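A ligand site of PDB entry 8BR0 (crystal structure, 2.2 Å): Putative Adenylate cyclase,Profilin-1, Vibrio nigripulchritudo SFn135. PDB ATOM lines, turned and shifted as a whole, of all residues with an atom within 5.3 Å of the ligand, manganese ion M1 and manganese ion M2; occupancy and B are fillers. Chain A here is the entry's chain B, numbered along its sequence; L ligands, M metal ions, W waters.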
ATOM      1  N   ARG A  60     -23.200  10.183  22.546  1.00  0.00           N
ATOM      2  CA  ARG A  60     -22.651   8.878  22.212  1.00  0.00           C
ATOM      3  C   ARG A  60     -22.390   8.055  23.493  1.00  0.00           C
ATOM      4  O   ARG A  60     -22.425   8.603  24.598  1.00  0.00           O
ATOM      5  CB  ARG A  60     -21.374   9.059  21.377  1.00  0.00           C
ATOM      6  CG  ARG A  60     -21.613   9.542  19.944  1.00  0.00           C
ATOM      7  CD  ARG A  60     -20.288   9.732  19.212  1.00  0.00           C
ATOM      8  NE  ARG A  60     -19.534   8.464  19.217  1.00  0.00           N
ATOM      9  CZ  ARG A  60     -18.264   8.331  19.586  1.00  0.00           C
ATOM     10  NH1 ARG A  60     -17.534   9.395  19.893  1.00  0.00           N
ATOM     11  NH2 ARG A  60     -17.710   7.129  19.607  1.00  0.00           N
ATOM     12  N   LYS A  78     -10.855  14.023  27.866  1.00  0.00           N
ATOM     13  CA  LYS A  78     -10.171  14.152  26.586  1.00  0.00           C
ATOM     14  C   LYS A  78     -10.904  14.938  25.501  1.00  0.00           C
ATOM     15  O   LYS A  78     -12.066  14.658  25.168  1.00  0.00           O
ATOM     16  CB  LYS A  78      -9.815  12.749  26.065  1.00  0.00           C
ATOM     17  CG  LYS A  78     -10.992  11.776  26.068  1.00  0.00           C
ATOM     18  CD  LYS A  78     -10.718  10.450  25.345  1.00  0.00           C
ATOM     19  CE  LYS A  78     -10.740  10.638  23.858  1.00  0.00           C
ATOM     20  NZ  LYS A  78     -10.633   9.322  23.125  1.00  0.00           N
ATOM     21  N   LEU A  80     -10.278  17.013  21.442  1.00  0.00           N
ATOM     22  CA  LEU A  80      -9.766  16.650  20.130  1.00  0.00           C
ATOM     23  C   LEU A  80      -8.229  16.518  20.080  1.00  0.00           C
ATOM     24  O   LEU A  80      -7.723  15.909  19.154  1.00  0.00           O
ATOM     25  CB  LEU A  80     -10.276  17.598  19.021  1.00  0.00           C
ATOM     26  CG  LEU A  80     -11.419  17.090  18.047  1.00  0.00           C
ATOM     27  CD1 LEU A  80     -12.379  16.111  18.666  1.00  0.00           C
ATOM     28  CD2 LEU A  80     -12.179  18.258  17.390  1.00  0.00           C
ATOM     29  N   VAL A  82      -6.496  14.763  22.278  1.00  0.00           N
ATOM     30  CA  VAL A  82      -6.209  13.456  22.855  1.00  0.00           C
ATOM     31  C   VAL A  82      -7.080  12.464  22.096  1.00  0.00           C
ATOM     32  O   VAL A  82      -8.240  12.237  22.432  1.00  0.00           O
ATOM     33  CB  VAL A  82      -6.379  13.414  24.408  1.00  0.00           C
ATOM     34  CG1 VAL A  82      -6.301  11.983  24.962  1.00  0.00           C
ATOM     35  CG2 VAL A  82      -5.335  14.312  25.084  1.00  0.00           C
ATOM     36  N   LYS A  83      -6.550  11.961  20.965  1.00  0.00           N
ATOM     37  CA  LYS A  83      -7.313  11.025  20.132  1.00  0.00           C
ATOM     38  C   LYS A  83      -7.210   9.557  20.595  1.00  0.00           C
ATOM     39  O   LYS A  83      -8.034   8.734  20.211  1.00  0.00           O
ATOM     40  CB  LYS A  83      -6.989  11.180  18.666  1.00  0.00           C
ATOM     41  CG  LYS A  83      -7.388  12.519  18.072  1.00  0.00           C
ATOM     42  CD  LYS A  83      -6.983  12.515  16.582  1.00  0.00           C
ATOM     43  CE  LYS A  83      -6.867  13.878  15.972  1.00  0.00           C
ATOM     44  NZ  LYS A  83      -7.855  14.793  16.557  1.00  0.00           N
ATOM     45  N   ALA A  84      -6.252   9.240  21.481  1.00  0.00           N
ATOM     46  CA  ALA A  84      -6.073   7.935  22.090  1.00  0.00           C
ATOM     47  C   ALA A  84      -7.361   7.520  22.815  1.00  0.00           C
ATOM     48  O   ALA A  84      -8.000   8.360  23.449  1.00  0.00           O
ATOM     49  CB  ALA A  84      -4.940   8.016  23.103  1.00  0.00           C
ATOM     50  N   LYS A  85      -7.799   6.266  22.643  1.00  0.00           N
ATOM     51  CA  LYS A  85      -9.029   5.794  23.275  1.00  0.00           C
ATOM     52  C   LYS A  85      -8.911   5.521  24.745  1.00  0.00           C
ATOM     53  O   LYS A  85      -7.835   5.158  25.248  1.00  0.00           O
ATOM     54  CB  LYS A  85      -9.567   4.528  22.584  1.00  0.00           C
ATOM     55  CG  LYS A  85      -9.859   4.708  21.109  1.00  0.00           C
ATOM     56  CD  LYS A  85     -10.933   5.732  20.877  1.00  0.00           C
ATOM     57  CE  LYS A  85     -11.408   5.685  19.449  1.00  0.00           C
ATOM     58  NZ  LYS A  85     -12.243   6.869  19.176  1.00  0.00           N
ATOM     59  N   SER A  86     -10.045   5.594  25.434  1.00  0.00           N
ATOM     60  CA  SER A  86     -10.107   5.209  26.832  1.00  0.00           C
ATOM     61  C   SER A  86     -10.171   3.664  26.884  1.00  0.00           C
ATOM     62  O   SER A  86     -10.418   3.006  25.871  1.00  0.00           O
ATOM     63  CB  SER A  86     -11.344   5.835  27.479  1.00  0.00           C
ATOM     64  OG  SER A  86     -12.532   5.148  27.138  1.00  0.00           O
ATOM     65  N   LYS A 104      -9.911   0.279  24.730  1.00  0.00           N
ATOM     66  CA  LYS A 104     -11.072  -0.419  24.227  1.00  0.00           C
ATOM     67  C   LYS A 104     -10.730  -1.109  22.882  1.00  0.00           C
ATOM     68  O   LYS A 104      -9.689  -0.818  22.274  1.00  0.00           O
ATOM     69  CB  LYS A 104     -12.246   0.558  24.103  1.00  0.00           C
ATOM     70  CG  LYS A 104     -12.032   1.587  23.008  1.00  0.00           C
ATOM     71  CD  LYS A 104     -13.223   2.471  22.828  1.00  0.00           C
ATOM     72  CE  LYS A 104     -13.351   3.411  23.981  1.00  0.00           C
ATOM     73  NZ  LYS A 104     -14.632   4.098  23.939  1.00  0.00           N
ATOM     74  N   ALA A 214     -12.946   9.656  29.743  1.00  0.00           N
ATOM     75  CA  ALA A 214     -13.633   9.843  28.478  1.00  0.00           C
ATOM     76  C   ALA A 214     -14.488  11.131  28.572  1.00  0.00           C
ATOM     77  O   ALA A 214     -14.834  11.606  29.668  1.00  0.00           O
ATOM     78  CB  ALA A 214     -14.539   8.659  28.237  1.00  0.00           C
ATOM     79  N   ASP A 215     -14.810  11.707  27.413  1.00  0.00           N
ATOM     80  CA  ASP A 215     -15.657  12.900  27.321  1.00  0.00           C
ATOM     81  C   ASP A 215     -17.111  12.489  27.026  1.00  0.00           C
ATOM     82  O   ASP A 215     -17.441  11.300  26.928  1.00  0.00           O
ATOM     83  CB  ASP A 215     -15.106  13.795  26.198  1.00  0.00           C
ATOM     84  CG  ASP A 215     -15.056  13.182  24.823  1.00  0.00           C
ATOM     85  OD1 ASP A 215     -14.785  11.969  24.713  1.00  0.00           O
ATOM     86  OD2 ASP A 215     -15.255  13.924  23.828  1.00  0.00           O
ATOM     87  N   ASP A 217     -19.449  12.803  24.051  1.00  0.00           N
ATOM     88  CA  ASP A 217     -19.439  13.174  22.655  1.00  0.00           C
ATOM     89  C   ASP A 217     -20.851  13.392  22.194  1.00  0.00           C
ATOM     90  O   ASP A 217     -21.609  12.429  22.153  1.00  0.00           O
ATOM     91  CB  ASP A 217     -18.829  12.077  21.816  1.00  0.00           C
ATOM     92  CG  ASP A 217     -17.362  11.918  22.025  1.00  0.00           C
ATOM     93  OD1 ASP A 217     -16.603  12.643  21.387  1.00  0.00           O
ATOM     94  OD2 ASP A 217     -16.964  11.058  22.810  1.00  0.00           O
ATOM     95  N   LEU A 274     -12.690  22.547  18.338  1.00  0.00           N
ATOM     96  CA  LEU A 274     -14.121  22.315  18.274  1.00  0.00           C
ATOM     97  C   LEU A 274     -14.514  21.442  17.110  1.00  0.00           C
ATOM     98  O   LEU A 274     -15.588  20.889  17.143  1.00  0.00           O
ATOM     99  CB  LEU A 274     -14.872  23.655  18.156  1.00  0.00           C
ATOM    100  CG  LEU A 274     -14.723  24.639  19.300  1.00  0.00           C
ATOM    101  CD1 LEU A 274     -15.390  25.951  18.952  1.00  0.00           C
ATOM    102  CD2 LEU A 274     -15.240  24.019  20.642  1.00  0.00           C
ATOM    103  N   GLY A 275     -13.706  21.380  16.052  1.00  0.00           N
ATOM    104  CA  GLY A 275     -14.042  20.644  14.853  1.00  0.00           C
ATOM    105  C   GLY A 275     -15.031  21.434  14.009  1.00  0.00           C
ATOM    106  O   GLY A 275     -14.982  22.673  13.960  1.00  0.00           O
ATOM    107  N   MET A 276     -15.934  20.747  13.345  1.00  0.00           N
ATOM    108  CA  MET A 276     -16.940  21.380  12.514  1.00  0.00           C
ATOM    109  C   MET A 276     -18.133  21.710  13.385  1.00  0.00           C
ATOM    110  O   MET A 276     -18.804  20.817  13.894  1.00  0.00           O
ATOM    111  CB  MET A 276     -17.344  20.440  11.392  1.00  0.00           C
ATOM    112  CG  MET A 276     -17.279  21.073  10.065  1.00  0.00           C
ATOM    113  SD  MET A 276     -15.616  21.072   9.460  1.00  0.00           S
ATOM    114  CE  MET A 276     -15.587  19.421   8.763  1.00  0.00           C
ATOM    115  N   HIS A 303     -16.155  19.481  21.876  1.00  0.00           N
ATOM    116  CA  HIS A 303     -16.168  19.747  20.441  1.00  0.00           C
ATOM    117  C   HIS A 303     -17.594  19.584  19.844  1.00  0.00           C
ATOM    118  O   HIS A 303     -18.533  19.271  20.559  1.00  0.00           O
ATOM    119  CB  HIS A 303     -15.141  18.784  19.753  1.00  0.00           C
ATOM    120  CG  HIS A 303     -15.284  17.337  20.128  1.00  0.00           C
ATOM    121  ND1 HIS A 303     -16.372  16.577  19.697  1.00  0.00           N
ATOM    122  CD2 HIS A 303     -14.506  16.571  20.934  1.00  0.00           C
ATOM    123  CE1 HIS A 303     -16.200  15.374  20.220  1.00  0.00           C
ATOM    124  NE2 HIS A 303     -15.094  15.310  20.976  1.00  0.00           N
ATOM    125  N   GLY A 304     -17.718  19.764  18.527  1.00  0.00           N
ATOM    126  CA  GLY A 304     -18.960  19.640  17.796  1.00  0.00           C
ATOM    127  C   GLY A 304     -19.525  18.235  17.768  1.00  0.00           C
ATOM    128  O   GLY A 304     -18.858  17.277  18.203  1.00  0.00           O
ATOM    129  N   ALA A 305     -20.745  18.112  17.213  1.00  0.00           N
ATOM    130  CA  ALA A 305     -21.444  16.849  17.147  1.00  0.00           C
ATOM    131  C   ALA A 305     -20.913  15.860  16.099  1.00  0.00           C
ATOM    132  O   ALA A 305     -20.255  16.251  15.114  1.00  0.00           O
ATOM    133  CB  ALA A 305     -22.946  17.070  16.970  1.00  0.00           C
ATOM    134  N   ASP A 306     -21.173  14.555  16.328  1.00  0.00           N
ATOM    135  CA  ASP A 306     -20.787  13.492  15.427  1.00  0.00           C
ATOM    136  C   ASP A 306     -21.430  13.648  14.048  1.00  0.00           C
ATOM    137  O   ASP A 306     -20.901  13.102  13.075  1.00  0.00           O
ATOM    138  CB  ASP A 306     -21.118  12.145  16.043  1.00  0.00           C
ATOM    139  CG  ASP A 306     -20.428  11.009  15.314  1.00  0.00           C
ATOM    140  OD1 ASP A 306     -19.182  10.956  15.349  1.00  0.00           O
ATOM    141  OD2 ASP A 306     -21.135  10.159  14.727  1.00  0.00           O
ATOM    142  N   ALA A 308     -21.328  16.157  12.185  1.00  0.00           N
ATOM    143  CA  ALA A 308     -20.414  16.892  11.319  1.00  0.00           C
ATOM    144  C   ALA A 308     -18.986  16.377  11.428  1.00  0.00           C
ATOM    145  O   ALA A 308     -18.078  17.076  11.033  1.00  0.00           O
ATOM    146  CB  ALA A 308     -20.423  18.350  11.697  1.00  0.00           C
ATOM    147  N   ASN A 309     -18.795  15.158  11.931  1.00  0.00           N
ATOM    148  CA  ASN A 309     -17.505  14.508  12.091  1.00  0.00           C
ATOM    149  C   ASN A 309     -17.247  13.641  10.861  1.00  0.00           C
ATOM    150  O   ASN A 309     -17.867  12.596  10.688  1.00  0.00           O
ATOM    151  CB  ASN A 309     -17.550  13.640  13.372  1.00  0.00           C
ATOM    152  CG  ASN A 309     -16.343  12.758  13.597  1.00  0.00           C
ATOM    153  OD1 ASN A 309     -15.301  12.882  12.951  1.00  0.00           O
ATOM    154  ND2 ASN A 309     -16.484  11.792  14.509  1.00  0.00           N
ATOM    155  N   PRO A 310     -16.265  14.041  10.013  1.00  0.00           N
ATOM    156  CA  PRO A 310     -15.954  13.222   8.835  1.00  0.00           C
ATOM    157  C   PRO A 310     -15.328  11.857   9.126  1.00  0.00           C
ATOM    158  O   PRO A 310     -15.220  11.028   8.220  1.00  0.00           O
ATOM    159  CB  PRO A 310     -15.015  14.117   8.021  1.00  0.00           C
ATOM    160  CG  PRO A 310     -14.407  15.015   8.998  1.00  0.00           C
ATOM    161  CD  PRO A 310     -15.431  15.250  10.067  1.00  0.00           C
ATOM    162  N   TYR A 311     -14.900  11.610  10.380  1.00  0.00           N
ATOM    163  CA  TYR A 311     -14.277  10.340  10.784  1.00  0.00           C
ATOM    164  C   TYR A 311     -15.215   9.504  11.672  1.00  0.00           C
ATOM    165  O   TYR A 311     -14.743   8.715  12.475  1.00  0.00           O
ATOM    166  CB  TYR A 311     -12.938  10.614  11.513  1.00  0.00           C
ATOM    167  CG  TYR A 311     -12.010  11.475  10.680  1.00  0.00           C
ATOM    168  CD1 TYR A 311     -11.392  10.954   9.545  1.00  0.00           C
ATOM    169  CD2 TYR A 311     -11.837  12.823  10.951  1.00  0.00           C
ATOM    170  CE1 TYR A 311     -10.587  11.744   8.738  1.00  0.00           C
ATOM    171  CE2 TYR A 311     -11.043  13.626  10.143  1.00  0.00           C
ATOM    172  CZ  TYR A 311     -10.411  13.074   9.036  1.00  0.00           C
ATOM    173  OH  TYR A 311      -9.612  13.858   8.218  1.00  0.00           O
ATOM    174  N   ASP A 316     -19.638   2.737  16.870  1.00  0.00           N
ATOM    175  CA  ASP A 316     -19.257   3.343  18.140  1.00  0.00           C
ATOM    176  C   ASP A 316     -20.191   4.455  18.633  1.00  0.00           C
ATOM    177  O   ASP A 316     -19.851   5.193  19.551  1.00  0.00           O
ATOM    178  CB  ASP A 316     -17.824   3.888  17.999  1.00  0.00           C
ATOM    179  CG  ASP A 316     -16.789   2.839  17.630  1.00  0.00           C
ATOM    180  OD1 ASP A 316     -17.089   1.623  17.781  1.00  0.00           O
ATOM    181  OD2 ASP A 316     -15.677   3.233  17.222  1.00  0.00           O
HETATM  182  N1  LIG L   1     -14.486  14.733  15.834  1.00  0.00           N
HETATM  183  C1  LIG L   1     -14.128  15.426  14.660  1.00  0.00           C
HETATM  184  N2  LIG L   1     -14.883  16.505  14.299  1.00  0.00           N
HETATM  185  C2  LIG L   1     -15.941  16.903  15.049  1.00  0.00           C
HETATM  186  C3  LIG L   1     -16.256  16.250  16.276  1.00  0.00           C
HETATM  187  C4  LIG L   1     -15.500  15.201  16.630  1.00  0.00           C
HETATM  188  O1  LIG L   1     -13.198  15.015  13.971  1.00  0.00           O
HETATM  189  N3  LIG L   1     -16.743  17.882  14.571  1.00  0.00           N
HETATM  190  C5  LIG L   1     -14.083  13.302  16.019  1.00  0.00           C
HETATM  191  C6  LIG L   1     -12.613  12.882  16.232  1.00  0.00           C
HETATM  192  O2  LIG L   1     -11.961  12.557  15.000  1.00  0.00           O
HETATM  193  C7  LIG L   1     -12.735  11.595  17.055  1.00  0.00           C
HETATM  194  C8  LIG L   1     -14.121  11.674  17.704  1.00  0.00           C
HETATM  195  O3  LIG L   1     -14.789  12.820  17.151  1.00  0.00           O
HETATM  196  C9  LIG L   1     -14.094  11.867  19.171  1.00  0.00           C
HETATM  197  O4  LIG L   1     -13.945  10.551  19.661  1.00  0.00           O
HETATM  198  P1  LIG L   1     -13.188  10.240  21.014  1.00  0.00           P
HETATM  199  O5  LIG L   1     -11.705  10.543  20.805  1.00  0.00           O
HETATM  200  O6  LIG L   1     -13.832  10.979  22.128  1.00  0.00           O
HETATM  201  O7  LIG L   1     -13.372   8.678  21.196  1.00  0.00           O
HETATM  202  P2  LIG L   1     -14.606   7.769  21.645  1.00  0.00           P
HETATM  203  O8  LIG L   1     -14.941   6.765  20.608  1.00  0.00           O
HETATM  204  O9  LIG L   1     -15.731   8.717  22.074  1.00  0.00           O
HETATM  205  O10 LIG L   1     -14.054   7.050  22.958  1.00  0.00           O
HETATM  206  P3  LIG L   1     -13.442   7.393  24.400  1.00  0.00           P
HETATM  207  O11 LIG L   1     -11.972   7.278  24.208  1.00  0.00           O
HETATM  208  O12 LIG L   1     -13.782   8.867  24.660  1.00  0.00           O
HETATM  209  O13 LIG L   1     -14.040   6.477  25.365  1.00  0.00           O
HETATM  210 MN    MN M   1     -15.352  10.134  23.662  1.00  0.00          MN
HETATM  211 MN    MN M   2     -14.646  13.216  21.769  1.00  0.00          MN
HETATM  212  O   HOH W   1     -16.844   9.092  25.063  1.00  0.00           O
HETATM  213  O   HOH W   2     -12.719  14.179  22.496  1.00  0.00           O
HETATM  214  O   HOH W   3     -10.737  13.109  21.058  1.00  0.00           O
HETATM  215  O   HOH W   4     -16.553   6.536  26.462  1.00  0.00           O
HETATM  216  O   HOH W   5     -10.330   9.084  19.139  1.00  0.00           O
HETATM  217  O   HOH W   6     -18.119   7.552  22.818  1.00  0.00           O
HETATM  218  O   HOH W   7     -10.703  14.704  14.929  1.00  0.00           O
HETATM  219  O   HOH W   8     -17.880  11.664  18.044  1.00  0.00           O
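NH2 of Arg 60 lies within salt-bridge range of O8 of the ligand (3.0 Å). The side-chain amino group (NZ) of Lys 78 is in salt-bridge range of an oxygen (O11) of the ligand, at 2.7 Å. The side-chain amide oxygen (OD1) of Asn 309 sits close to an oxygen (O1) of the ligand (3.2 Å). An oxygen (O13) of the ligand is in salt-bridge range of the side-chain amino group (NZ) of Lys 104, 2.8 Å away. An oxygen (O13) of the ligand sits at hydrogen-bond distance from the side-chain hydroxyl (OG) of Ser 86 (2.7 Å). The side-chain amino group (NZ) of Lys 85 lies within salt-bridge range of an oxygen (O8) of the ligand (3.1 Å). The backbone NH (N) of Ser 86 lies within hydrogen-bond range of an oxygen (O11) of the ligand (2.8 Å).
The backbone carbonyl oxygen of Leu 80 lies within hydrogen-bond range of the side-chain amino group of Lys 83. NH2 of Arg 60 is in hydrogen-bond range of O of Asp 316 (2.9 Å). The backbone carbonyl oxygen of Asp 217 is in hydrogen-bond range of the backbone NH of Arg 60 (2.8 Å). The backbone carbonyl oxygen (O) of Ala 84 lies within hydrogen-bond range of the side-chain amino group (NZ) of Lys 78. The backbone NH (N) of Gly 304 lies within hydrogen-bond range of the backbone carbonyl oxygen (O) of Leu 274 (2.8 Å). O of Ser 86 lies within hydrogen-bond range of N of Lys 104 (3.0 Å). ND2 of Asn 309 is in hydrogen-bond range of OD1 of Asp 306 (2.9 Å). The side-chain amide oxygen of Asn 309 is in hydrogen-bond range of the backbone NH of Tyr 311 (2.9 Å).
N3 of the ligand lies close to N of Met 276, 3.2 Å away. Merely in contact with the ligand: Gly 304, Ala 214, Leu 80, Ala 308, Gly 275, Ala 305 and Tyr 311. Hydrophobic or aromatic side chains that line the ligand: Leu 80, Ala 214, His 303 and Tyr 311. 17 residues have an atom within 4 Å of the ligand: Arg 60, Lys 78, Leu 80, Lys 85, Ser 86, Lys 104, Ala 214, Asp 215, Asp 217, Gly 275, Met 276, His 303, Gly 304, Ala 305, Ala 308, Asn 309 and Tyr 311.
Two residues have an atom within 4 Å of manganese ion M1: Asp 215 and Asp 217.
Three residues have an atom within 4 Å of manganese ion M2: Asp 215, Asp 217 and His 303. The nearest printed residue that does not touch manganese ion M2 is Lys 78 (4.5 Å).
OD2 of Asp 217 is bound to manganese ion M1, 2.0 Å away. O9 of the ligand is bound to manganese ion M1 (2.2 Å). OD1 of Asp 215 is bound to manganese ion M1. O12 of the ligand is bound to manganese ion M1 (2.3 Å). Manganese ion M1 is bound by water W1 (2.3 Å). O6 of the ligand is bound to manganese ion M1 (2.3 Å). Manganese ion M1 has six donor atoms within binding distance.
Manganese ion M2 is bound by OD1 of Asp 217, OD2 of Asp 215, water W2, NE2 of His 303 and O6 of the ligand.
Water W7 lies within hydrogen-bond range of an oxygen (O2) of the ligand and the side-chain amino group of Lys 83. Water W5 lies within hydrogen-bond range of the backbone carbonyl oxygen (O) of Lys 83 (2.6 Å), an oxygen (O5) of the ligand (2.6 Å) and the side-chain amino group (NZ) of Lys 85 (2.9 Å). Water W3 bridges O5 of the ligand (2.8 Å) and O of Val 82 (3.0 Å). Water W8 lies within hydrogen-bond range of NH1 of Arg 60 (2.9 Å), OD1 of Asp 306 (3.1 Å) and O3 of the ligand (3.4 Å).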
